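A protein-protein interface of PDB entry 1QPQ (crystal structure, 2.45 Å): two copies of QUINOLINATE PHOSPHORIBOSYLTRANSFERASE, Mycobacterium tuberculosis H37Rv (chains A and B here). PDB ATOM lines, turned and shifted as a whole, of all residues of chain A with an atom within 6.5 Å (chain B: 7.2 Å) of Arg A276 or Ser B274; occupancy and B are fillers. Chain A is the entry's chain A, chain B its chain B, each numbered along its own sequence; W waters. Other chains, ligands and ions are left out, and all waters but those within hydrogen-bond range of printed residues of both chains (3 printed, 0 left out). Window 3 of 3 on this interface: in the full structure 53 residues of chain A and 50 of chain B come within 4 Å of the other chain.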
ATOM      1  N   GLU A  48      30.896 -19.370  -8.903  1.00  0.00           N
ATOM      2  CA  GLU A  48      29.466 -19.393  -8.849  1.00  0.00           C
ATOM      3  C   GLU A  48      28.850 -19.093 -10.191  1.00  0.00           C
ATOM      4  O   GLU A  48      29.563 -18.759 -11.133  1.00  0.00           O
ATOM      5  CB  GLU A  48      28.960 -18.442  -7.771  1.00  0.00           C
ATOM      6  CG  GLU A  48      29.333 -16.980  -7.896  1.00  0.00           C
ATOM      7  CD  GLU A  48      29.055 -16.185  -6.602  1.00  0.00           C
ATOM      8  OE1 GLU A  48      28.583 -16.773  -5.609  1.00  0.00           O
ATOM      9  OE2 GLU A  48      29.325 -14.970  -6.552  1.00  0.00           O
ATOM     10  N   ALA A  49      27.542 -19.299 -10.311  1.00  0.00           N
ATOM     11  CA  ALA A  49      26.844 -19.069 -11.577  1.00  0.00           C
ATOM     12  C   ALA A  49      26.465 -17.618 -11.747  1.00  0.00           C
ATOM     13  O   ALA A  49      26.323 -16.879 -10.765  1.00  0.00           O
ATOM     14  CB  ALA A  49      25.612 -19.931 -11.682  1.00  0.00           C
ATOM     15  N   GLY A 111      34.735  -9.142 -11.738  1.00  0.00           N
ATOM     16  CA  GLY A 111      33.842  -9.652 -10.722  1.00  0.00           C
ATOM     17  C   GLY A 111      32.747  -8.611 -10.514  1.00  0.00           C
ATOM     18  O   GLY A 111      31.576  -8.971 -10.401  1.00  0.00           O
ATOM     19  N   HIS A 112      33.116  -7.327 -10.469  1.00  0.00           N
ATOM     20  CA  HIS A 112      32.137  -6.257 -10.287  1.00  0.00           C
ATOM     21  C   HIS A 112      31.165  -6.146 -11.472  1.00  0.00           C
ATOM     22  O   HIS A 112      29.948  -6.113 -11.320  1.00  0.00           O
ATOM     23  CB  HIS A 112      32.850  -4.930 -10.100  1.00  0.00           C
ATOM     24  CG  HIS A 112      31.930  -3.774  -9.843  1.00  0.00           C
ATOM     25  ND1 HIS A 112      31.356  -3.535  -8.616  1.00  0.00           N
ATOM     26  CD2 HIS A 112      31.527  -2.761 -10.647  1.00  0.00           C
ATOM     27  CE1 HIS A 112      30.648  -2.426  -8.666  1.00  0.00           C
ATOM     28  NE2 HIS A 112      30.736  -1.938  -9.891  1.00  0.00           N
ATOM     29  N   SER A 114      30.538  -8.366 -13.618  1.00  0.00           N
ATOM     30  CA  SER A 114      29.738  -9.581 -13.804  1.00  0.00           C
ATOM     31  C   SER A 114      28.599  -9.590 -12.774  1.00  0.00           C
ATOM     32  O   SER A 114      27.492  -9.970 -13.089  1.00  0.00           O
ATOM     33  CB  SER A 114      30.593 -10.824 -13.689  1.00  0.00           C
ATOM     34  OG  SER A 114      31.438 -10.887 -14.810  1.00  0.00           O
ATOM     35  N   GLY A 115      28.852  -9.081 -11.571  1.00  0.00           N
ATOM     36  CA  GLY A 115      27.826  -9.007 -10.557  1.00  0.00           C
ATOM     37  C   GLY A 115      26.673  -8.173 -11.107  1.00  0.00           C
ATOM     38  O   GLY A 115      25.527  -8.565 -10.951  1.00  0.00           O
ATOM     39  N   ILE A 116      26.979  -7.040 -11.760  1.00  0.00           N
ATOM     40  CA  ILE A 116      25.994  -6.122 -12.370  1.00  0.00           C
ATOM     41  C   ILE A 116      25.206  -6.771 -13.502  1.00  0.00           C
ATOM     42  O   ILE A 116      24.002  -6.704 -13.500  1.00  0.00           O
ATOM     43  CB  ILE A 116      26.661  -4.830 -12.929  1.00  0.00           C
ATOM     44  CG1 ILE A 116      27.125  -3.909 -11.806  1.00  0.00           C
ATOM     45  CG2 ILE A 116      25.696  -4.068 -13.762  1.00  0.00           C
ATOM     46  CD1 ILE A 116      28.054  -2.805 -12.301  1.00  0.00           C
ATOM     47  N   THR A 118      24.838  -9.923 -14.021  1.00  0.00           N
ATOM     48  CA  THR A 118      24.124 -11.052 -13.422  1.00  0.00           C
ATOM     49  C   THR A 118      22.792 -10.531 -12.867  1.00  0.00           C
ATOM     50  O   THR A 118      21.738 -11.054 -13.206  1.00  0.00           O
ATOM     51  CB  THR A 118      24.975 -11.713 -12.297  1.00  0.00           C
ATOM     52  OG1 THR A 118      26.172 -12.223 -12.862  1.00  0.00           O
ATOM     53  CG2 THR A 118      24.264 -12.900 -11.670  1.00  0.00           C
ATOM     54  N   HIS A 273      24.315   0.661  -7.725  1.00  0.00           N
ATOM     55  CA  HIS A 273      24.715   0.966  -6.342  1.00  0.00           C
ATOM     56  C   HIS A 273      24.414  -0.388  -5.708  1.00  0.00           C
ATOM     57  O   HIS A 273      23.745  -1.202  -6.326  1.00  0.00           O
ATOM     58  CB  HIS A 273      23.892   2.117  -5.727  1.00  0.00           C
ATOM     59  CG  HIS A 273      22.415   1.850  -5.531  1.00  0.00           C
ATOM     60  ND1 HIS A 273      21.927   0.902  -4.655  1.00  0.00           N
ATOM     61  CD2 HIS A 273      21.331   2.545  -5.955  1.00  0.00           C
ATOM     62  CE1 HIS A 273      20.619   1.031  -4.538  1.00  0.00           C
ATOM     63  NE2 HIS A 273      20.232   2.022  -5.314  1.00  0.00           N
ATOM     64  N   SER A 274      24.892  -0.722  -4.546  1.00  0.00           N
ATOM     65  CA  SER A 274      24.468  -2.071  -4.098  1.00  0.00           C
ATOM     66  C   SER A 274      24.743  -3.265  -5.026  1.00  0.00           C
ATOM     67  O   SER A 274      23.829  -4.076  -5.245  1.00  0.00           O
ATOM     68  CB  SER A 274      22.948  -2.148  -3.795  1.00  0.00           C
ATOM     69  OG  SER A 274      22.529  -1.264  -2.754  1.00  0.00           O
ATOM     70  N   VAL A 275      25.951  -3.417  -5.566  1.00  0.00           N
ATOM     71  CA  VAL A 275      26.182  -4.605  -6.397  1.00  0.00           C
ATOM     72  C   VAL A 275      26.931  -5.701  -5.627  1.00  0.00           C
ATOM     73  O   VAL A 275      27.777  -5.414  -4.787  1.00  0.00           O
ATOM     74  CB  VAL A 275      26.863  -4.314  -7.801  1.00  0.00           C
ATOM     75  CG1 VAL A 275      27.014  -2.855  -8.070  1.00  0.00           C
ATOM     76  CG2 VAL A 275      28.179  -5.022  -7.934  1.00  0.00           C
ATOM     77  N   ARG A 276      26.596  -6.960  -5.903  1.00  0.00           N
ATOM     78  CA  ARG A 276      27.215  -8.100  -5.251  1.00  0.00           C
ATOM     79  C   ARG A 276      28.123  -8.715  -6.267  1.00  0.00           C
ATOM     80  O   ARG A 276      27.688  -9.080  -7.342  1.00  0.00           O
ATOM     81  CB  ARG A 276      26.163  -9.124  -4.885  1.00  0.00           C
ATOM     82  CG  ARG A 276      26.458  -9.874  -3.610  1.00  0.00           C
ATOM     83  CD  ARG A 276      25.641 -11.128  -3.545  1.00  0.00           C
ATOM     84  NE  ARG A 276      26.004 -12.017  -4.641  1.00  0.00           N
ATOM     85  CZ  ARG A 276      26.476 -13.251  -4.483  1.00  0.00           C
ATOM     86  NH1 ARG A 276      26.637 -13.753  -3.261  1.00  0.00           N
ATOM     87  NH2 ARG A 276      26.809 -13.978  -5.551  1.00  0.00           N
ATOM     88  N   VAL A 277      29.374  -8.904  -5.888  1.00  0.00           N
ATOM     89  CA  VAL A 277      30.370  -9.450  -6.795  1.00  0.00           C
ATOM     90  C   VAL A 277      30.139 -10.857  -7.313  1.00  0.00           C
ATOM     91  O   VAL A 277      29.624 -11.692  -6.583  1.00  0.00           O
ATOM     92  CB  VAL A 277      31.777  -9.426  -6.112  1.00  0.00           C
ATOM     93  CG1 VAL A 277      31.955 -10.596  -5.170  1.00  0.00           C
ATOM     94  CG2 VAL A 277      32.858  -9.425  -7.134  1.00  0.00           C
ATOM     95  N   LEU A 278      30.443 -11.104  -8.586  1.00  0.00           N
ATOM     96  CA  LEU A 278      30.380 -12.460  -9.077  1.00  0.00           C
ATOM     97  C   LEU A 278      31.759 -13.004  -8.667  1.00  0.00           C
ATOM     98  O   LEU A 278      32.797 -12.477  -9.080  1.00  0.00           O
ATOM     99  CB  LEU A 278      30.243 -12.548 -10.598  1.00  0.00           C
ATOM    100  CG  LEU A 278      29.994 -14.011 -11.052  1.00  0.00           C
ATOM    101  CD1 LEU A 278      28.705 -14.554 -10.461  1.00  0.00           C
ATOM    102  CD2 LEU A 278      29.955 -14.137 -12.554  1.00  0.00           C
ATOM    103  N   ASP A 279      31.769 -14.029  -7.833  1.00  0.00           N
ATOM    104  CA  ASP A 279      33.008 -14.641  -7.367  1.00  0.00           C
ATOM    105  C   ASP A 279      33.711 -15.414  -8.468  1.00  0.00           C
ATOM    106  O   ASP A 279      33.210 -16.420  -8.965  1.00  0.00           O
ATOM    107  CB  ASP A 279      32.717 -15.562  -6.194  1.00  0.00           C
ATOM    108  CG  ASP A 279      33.921 -15.848  -5.368  1.00  0.00           C
ATOM    109  OD1 ASP A 279      34.975 -15.220  -5.583  1.00  0.00           O
ATOM    110  OD2 ASP A 279      33.793 -16.701  -4.473  1.00  0.00           O
ATOM    111  N   HIS B 112      27.702   5.142  -0.559  1.00  0.00           N
ATOM    112  CA  HIS B 112      28.562   3.974  -0.726  1.00  0.00           C
ATOM    113  C   HIS B 112      29.361   3.749   0.536  1.00  0.00           C
ATOM    114  O   HIS B 112      29.314   2.662   1.121  1.00  0.00           O
ATOM    115  CB  HIS B 112      29.517   4.121  -1.916  1.00  0.00           C
ATOM    116  CG  HIS B 112      30.386   2.916  -2.158  1.00  0.00           C
ATOM    117  ND1 HIS B 112      29.934   1.775  -2.796  1.00  0.00           N
ATOM    118  CD2 HIS B 112      31.682   2.675  -1.851  1.00  0.00           C
ATOM    119  CE1 HIS B 112      30.909   0.887  -2.871  1.00  0.00           C
ATOM    120  NE2 HIS B 112      31.982   1.409  -2.303  1.00  0.00           N
ATOM    121  N   ALA B 119      27.920  -2.028   7.201  1.00  0.00           N
ATOM    122  CA  ALA B 119      28.161  -3.442   7.143  1.00  0.00           C
ATOM    123  C   ALA B 119      29.218  -3.854   8.120  1.00  0.00           C
ATOM    124  O   ALA B 119      29.007  -4.791   8.876  1.00  0.00           O
ATOM    125  CB  ALA B 119      28.607  -3.804   5.790  1.00  0.00           C
ATOM    126  N   LYS B 139      40.131  -6.647  -2.125  1.00  0.00           N
ATOM    127  CA  LYS B 139      39.005  -6.794  -3.064  1.00  0.00           C
ATOM    128  C   LYS B 139      38.182  -5.503  -3.005  1.00  0.00           C
ATOM    129  O   LYS B 139      37.067  -5.484  -2.488  1.00  0.00           O
ATOM    130  CB  LYS B 139      38.160  -7.983  -2.679  1.00  0.00           C
ATOM    131  CG  LYS B 139      38.988  -9.186  -2.546  1.00  0.00           C
ATOM    132  CD  LYS B 139      38.163 -10.356  -2.158  1.00  0.00           C
ATOM    133  CE  LYS B 139      39.050 -11.528  -1.755  1.00  0.00           C
ATOM    134  NZ  LYS B 139      38.362 -12.801  -2.114  1.00  0.00           N
ATOM    135  N   LEU B 141      37.350  -1.500  -5.128  1.00  0.00           N
ATOM    136  CA  LEU B 141      37.049  -1.065  -6.487  1.00  0.00           C
ATOM    137  C   LEU B 141      38.179  -0.160  -6.941  1.00  0.00           C
ATOM    138  O   LEU B 141      38.597   0.713  -6.195  1.00  0.00           O
ATOM    139  CB  LEU B 141      35.722  -0.332  -6.519  1.00  0.00           C
ATOM    140  CG  LEU B 141      34.443  -1.104  -6.850  1.00  0.00           C
ATOM    141  CD1 LEU B 141      34.777  -2.384  -7.570  1.00  0.00           C
ATOM    142  CD2 LEU B 141      33.626  -1.378  -5.619  1.00  0.00           C
ATOM    143  N   GLY B 269      35.965 -10.026   2.681  1.00  0.00           N
ATOM    144  CA  GLY B 269      36.000  -9.380   1.401  1.00  0.00           C
ATOM    145  C   GLY B 269      34.722  -8.616   1.088  1.00  0.00           C
ATOM    146  O   GLY B 269      34.764  -7.521   0.492  1.00  0.00           O
ATOM    147  N   ALA B 270      33.584  -9.180   1.481  1.00  0.00           N
ATOM    148  CA  ALA B 270      32.288  -8.567   1.207  1.00  0.00           C
ATOM    149  C   ALA B 270      32.149  -7.150   1.748  1.00  0.00           C
ATOM    150  O   ALA B 270      31.279  -6.418   1.347  1.00  0.00           O
ATOM    151  CB  ALA B 270      31.197  -9.422   1.752  1.00  0.00           C
ATOM    152  N   LEU B 271      32.925  -6.803   2.748  1.00  0.00           N
ATOM    153  CA  LEU B 271      32.856  -5.470   3.290  1.00  0.00           C
ATOM    154  C   LEU B 271      33.093  -4.454   2.167  1.00  0.00           C
ATOM    155  O   LEU B 271      32.486  -3.376   2.177  1.00  0.00           O
ATOM    156  CB  LEU B 271      33.961  -5.304   4.301  1.00  0.00           C
ATOM    157  CG  LEU B 271      33.604  -5.249   5.758  1.00  0.00           C
ATOM    158  CD1 LEU B 271      32.409  -6.070   6.046  1.00  0.00           C
ATOM    159  CD2 LEU B 271      34.831  -5.678   6.527  1.00  0.00           C
ATOM    160  N   THR B 272      33.952  -4.801   1.196  1.00  0.00           N
ATOM    161  CA  THR B 272      34.301  -3.894   0.095  1.00  0.00           C
ATOM    162  C   THR B 272      33.772  -4.279  -1.284  1.00  0.00           C
ATOM    163  O   THR B 272      33.459  -3.391  -2.104  1.00  0.00           O
ATOM    164  CB  THR B 272      35.780  -3.669   0.074  1.00  0.00           C
ATOM    165  OG1 THR B 272      36.430  -4.913  -0.164  1.00  0.00           O
ATOM    166  CG2 THR B 272      36.219  -3.145   1.423  1.00  0.00           C
ATOM    167  N   HIS B 273      33.759  -5.565  -1.614  1.00  0.00           N
ATOM    168  CA  HIS B 273      33.103  -5.967  -2.879  1.00  0.00           C
ATOM    169  C   HIS B 273      31.641  -6.199  -2.400  1.00  0.00           C
ATOM    170  O   HIS B 273      31.396  -6.206  -1.197  1.00  0.00           O
ATOM    171  CB  HIS B 273      33.742  -7.231  -3.493  1.00  0.00           C
ATOM    172  CG  HIS B 273      33.561  -8.497  -2.693  1.00  0.00           C
ATOM    173  ND1 HIS B 273      32.326  -9.084  -2.473  1.00  0.00           N
ATOM    174  CD2 HIS B 273      34.470  -9.324  -2.126  1.00  0.00           C
ATOM    175  CE1 HIS B 273      32.484 -10.212  -1.810  1.00  0.00           C
ATOM    176  NE2 HIS B 273      33.773 -10.381  -1.589  1.00  0.00           N
ATOM    177  N   SER B 274      30.635  -6.344  -3.240  1.00  0.00           N
ATOM    178  CA  SER B 274      29.304  -6.569  -2.598  1.00  0.00           C
ATOM    179  C   SER B 274      28.833  -5.547  -1.511  1.00  0.00           C
ATOM    180  O   SER B 274      28.409  -5.957  -0.427  1.00  0.00           O
ATOM    181  CB  SER B 274      29.211  -7.978  -1.948  1.00  0.00           C
ATOM    182  OG  SER B 274      29.602  -9.032  -2.836  1.00  0.00           O
ATOM    183  N   VAL B 275      28.887  -4.242  -1.754  1.00  0.00           N
ATOM    184  CA  VAL B 275      28.376  -3.334  -0.728  1.00  0.00           C
ATOM    185  C   VAL B 275      26.973  -2.821  -1.122  1.00  0.00           C
ATOM    186  O   VAL B 275      26.680  -2.619  -2.317  1.00  0.00           O
ATOM    187  CB  VAL B 275      29.339  -2.146  -0.361  1.00  0.00           C
ATOM    188  CG1 VAL B 275      30.665  -2.238  -1.085  1.00  0.00           C
ATOM    189  CG2 VAL B 275      28.649  -0.784  -0.596  1.00  0.00           C
ATOM    190  N   ARG B 276      26.118  -2.634  -0.115  1.00  0.00           N
ATOM    191  CA  ARG B 276      24.759  -2.167  -0.305  1.00  0.00           C
ATOM    192  C   ARG B 276      24.709  -0.748   0.203  1.00  0.00           C
ATOM    193  O   ARG B 276      25.024  -0.457   1.338  1.00  0.00           O
ATOM    194  CB  ARG B 276      23.785  -3.020   0.485  1.00  0.00           C
ATOM    195  CG  ARG B 276      22.462  -3.135  -0.154  1.00  0.00           C
ATOM    196  CD  ARG B 276      21.454  -3.532   0.861  1.00  0.00           C
ATOM    197  NE  ARG B 276      21.312  -2.497   1.884  1.00  0.00           N
ATOM    198  CZ  ARG B 276      20.156  -1.929   2.219  1.00  0.00           C
ATOM    199  NH1 ARG B 276      19.028  -2.289   1.605  1.00  0.00           N
ATOM    200  NH2 ARG B 276      20.126  -1.013   3.186  1.00  0.00           N
HETATM  201  O   HOH W   1      27.948  -1.366  -4.619  1.00  0.00           O
HETATM  202  O   HOH W   2      31.758  -5.492  -6.364  1.00  0.00           O
HETATM  203  O   HOH W   3      26.747   1.586  -3.481  1.00  0.00           O
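Ser A274 touches Val B275, and with the chains exchanged Val A275 touches Ser B274. Ser A274 touches Arg B276, and with the chains exchanged Arg A276 touches Ser B274. Val A275 touches its own counterpart, Val B275. Positions printed for both chains: 112, 273, 274, 275 and 276.
Hydrophobic or aromatic side chains of chain A within 4 Å of the printed part of chain B: His A112 and Val A277. Along chain A the printed residues that touch a printed residue of chain B span positions 112 to 277. Among the printed residues, 8 pairs touch across the chains. Among the printed residues, no Asp or Glu carboxylate lies within 4 Å of a Lys or Arg side-chain nitrogen of the other chain.
Of the printed residues of chain B, Ser A274 touches Val B275 (2.9 Å) and Arg B276 (3.2 Å). Of chain B, only Ser B274 (3.3 Å) comes within 4 Å of Arg A276. His B112 touches none of the printed residues of chain A. Ser B274 touches just these residues of chain A: Val A275 (2.9 Å), Arg A276 (3.3 Å) and Val A277 (3.1 Å). Of the printed residues of chain A, Val B275 touches Ser A274 and Val A275. The nearest residue of chain A that does not touch Ser B274 is Ser A274 (5.9 Å).
The side-chain carboxylate of Glu A48 is in salt-bridge range of the guanidinium group of Arg A276, at 2.9 Å. A ring nitrogen (ND1) of His A273 sits at hydrogen-bond distance from the side-chain hydroxyl (OG) of Ser A274, 2.9 Å away. The backbone carbonyl oxygen of Lys B139 sits at hydrogen-bond distance from the backbone NH of His B273, at 3.4 Å. NE2 of His B273 is in hydrogen-bond range of N of Ala B270. ND1 of His B273 is in hydrogen-bond range of OG of Ser B274 (2.7 Å).
Leu B141 touches His A112. Arg B276 touches Ser A274. CG of Arg A276 touches OG of Ser B274 (3.3 Å). His B273 touches Val A277.
Water W1 lies within hydrogen-bond range of the backbone carbonyl oxygen of Val B275 (2.9 Å), the backbone NH of Val A275 (3.0 Å) and the backbone NH of Ser A274 (3.1 Å). Water W2 lies within hydrogen-bond range of ND1 of His A112 (3.0 Å) and N of Ser B274 (3.4 Å). Water W3 bridges N of Ser A274 and ND1 of His B112.
O of Val B275 lies close to N of Ser A274. The backbone NH (N) of Ser B274 sits close to the backbone carbonyl oxygen (O) of Val A275 (3.4 Å). The backbone NH (N) of Val A275 lies within hydrogen-bond range of the backbone carbonyl oxygen (O) of Val B275, at 3.4 Å. The side-chain hydroxyl of Ser B274 sits at hydrogen-bond distance from the backbone NH of Val A277 (3.1 Å).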
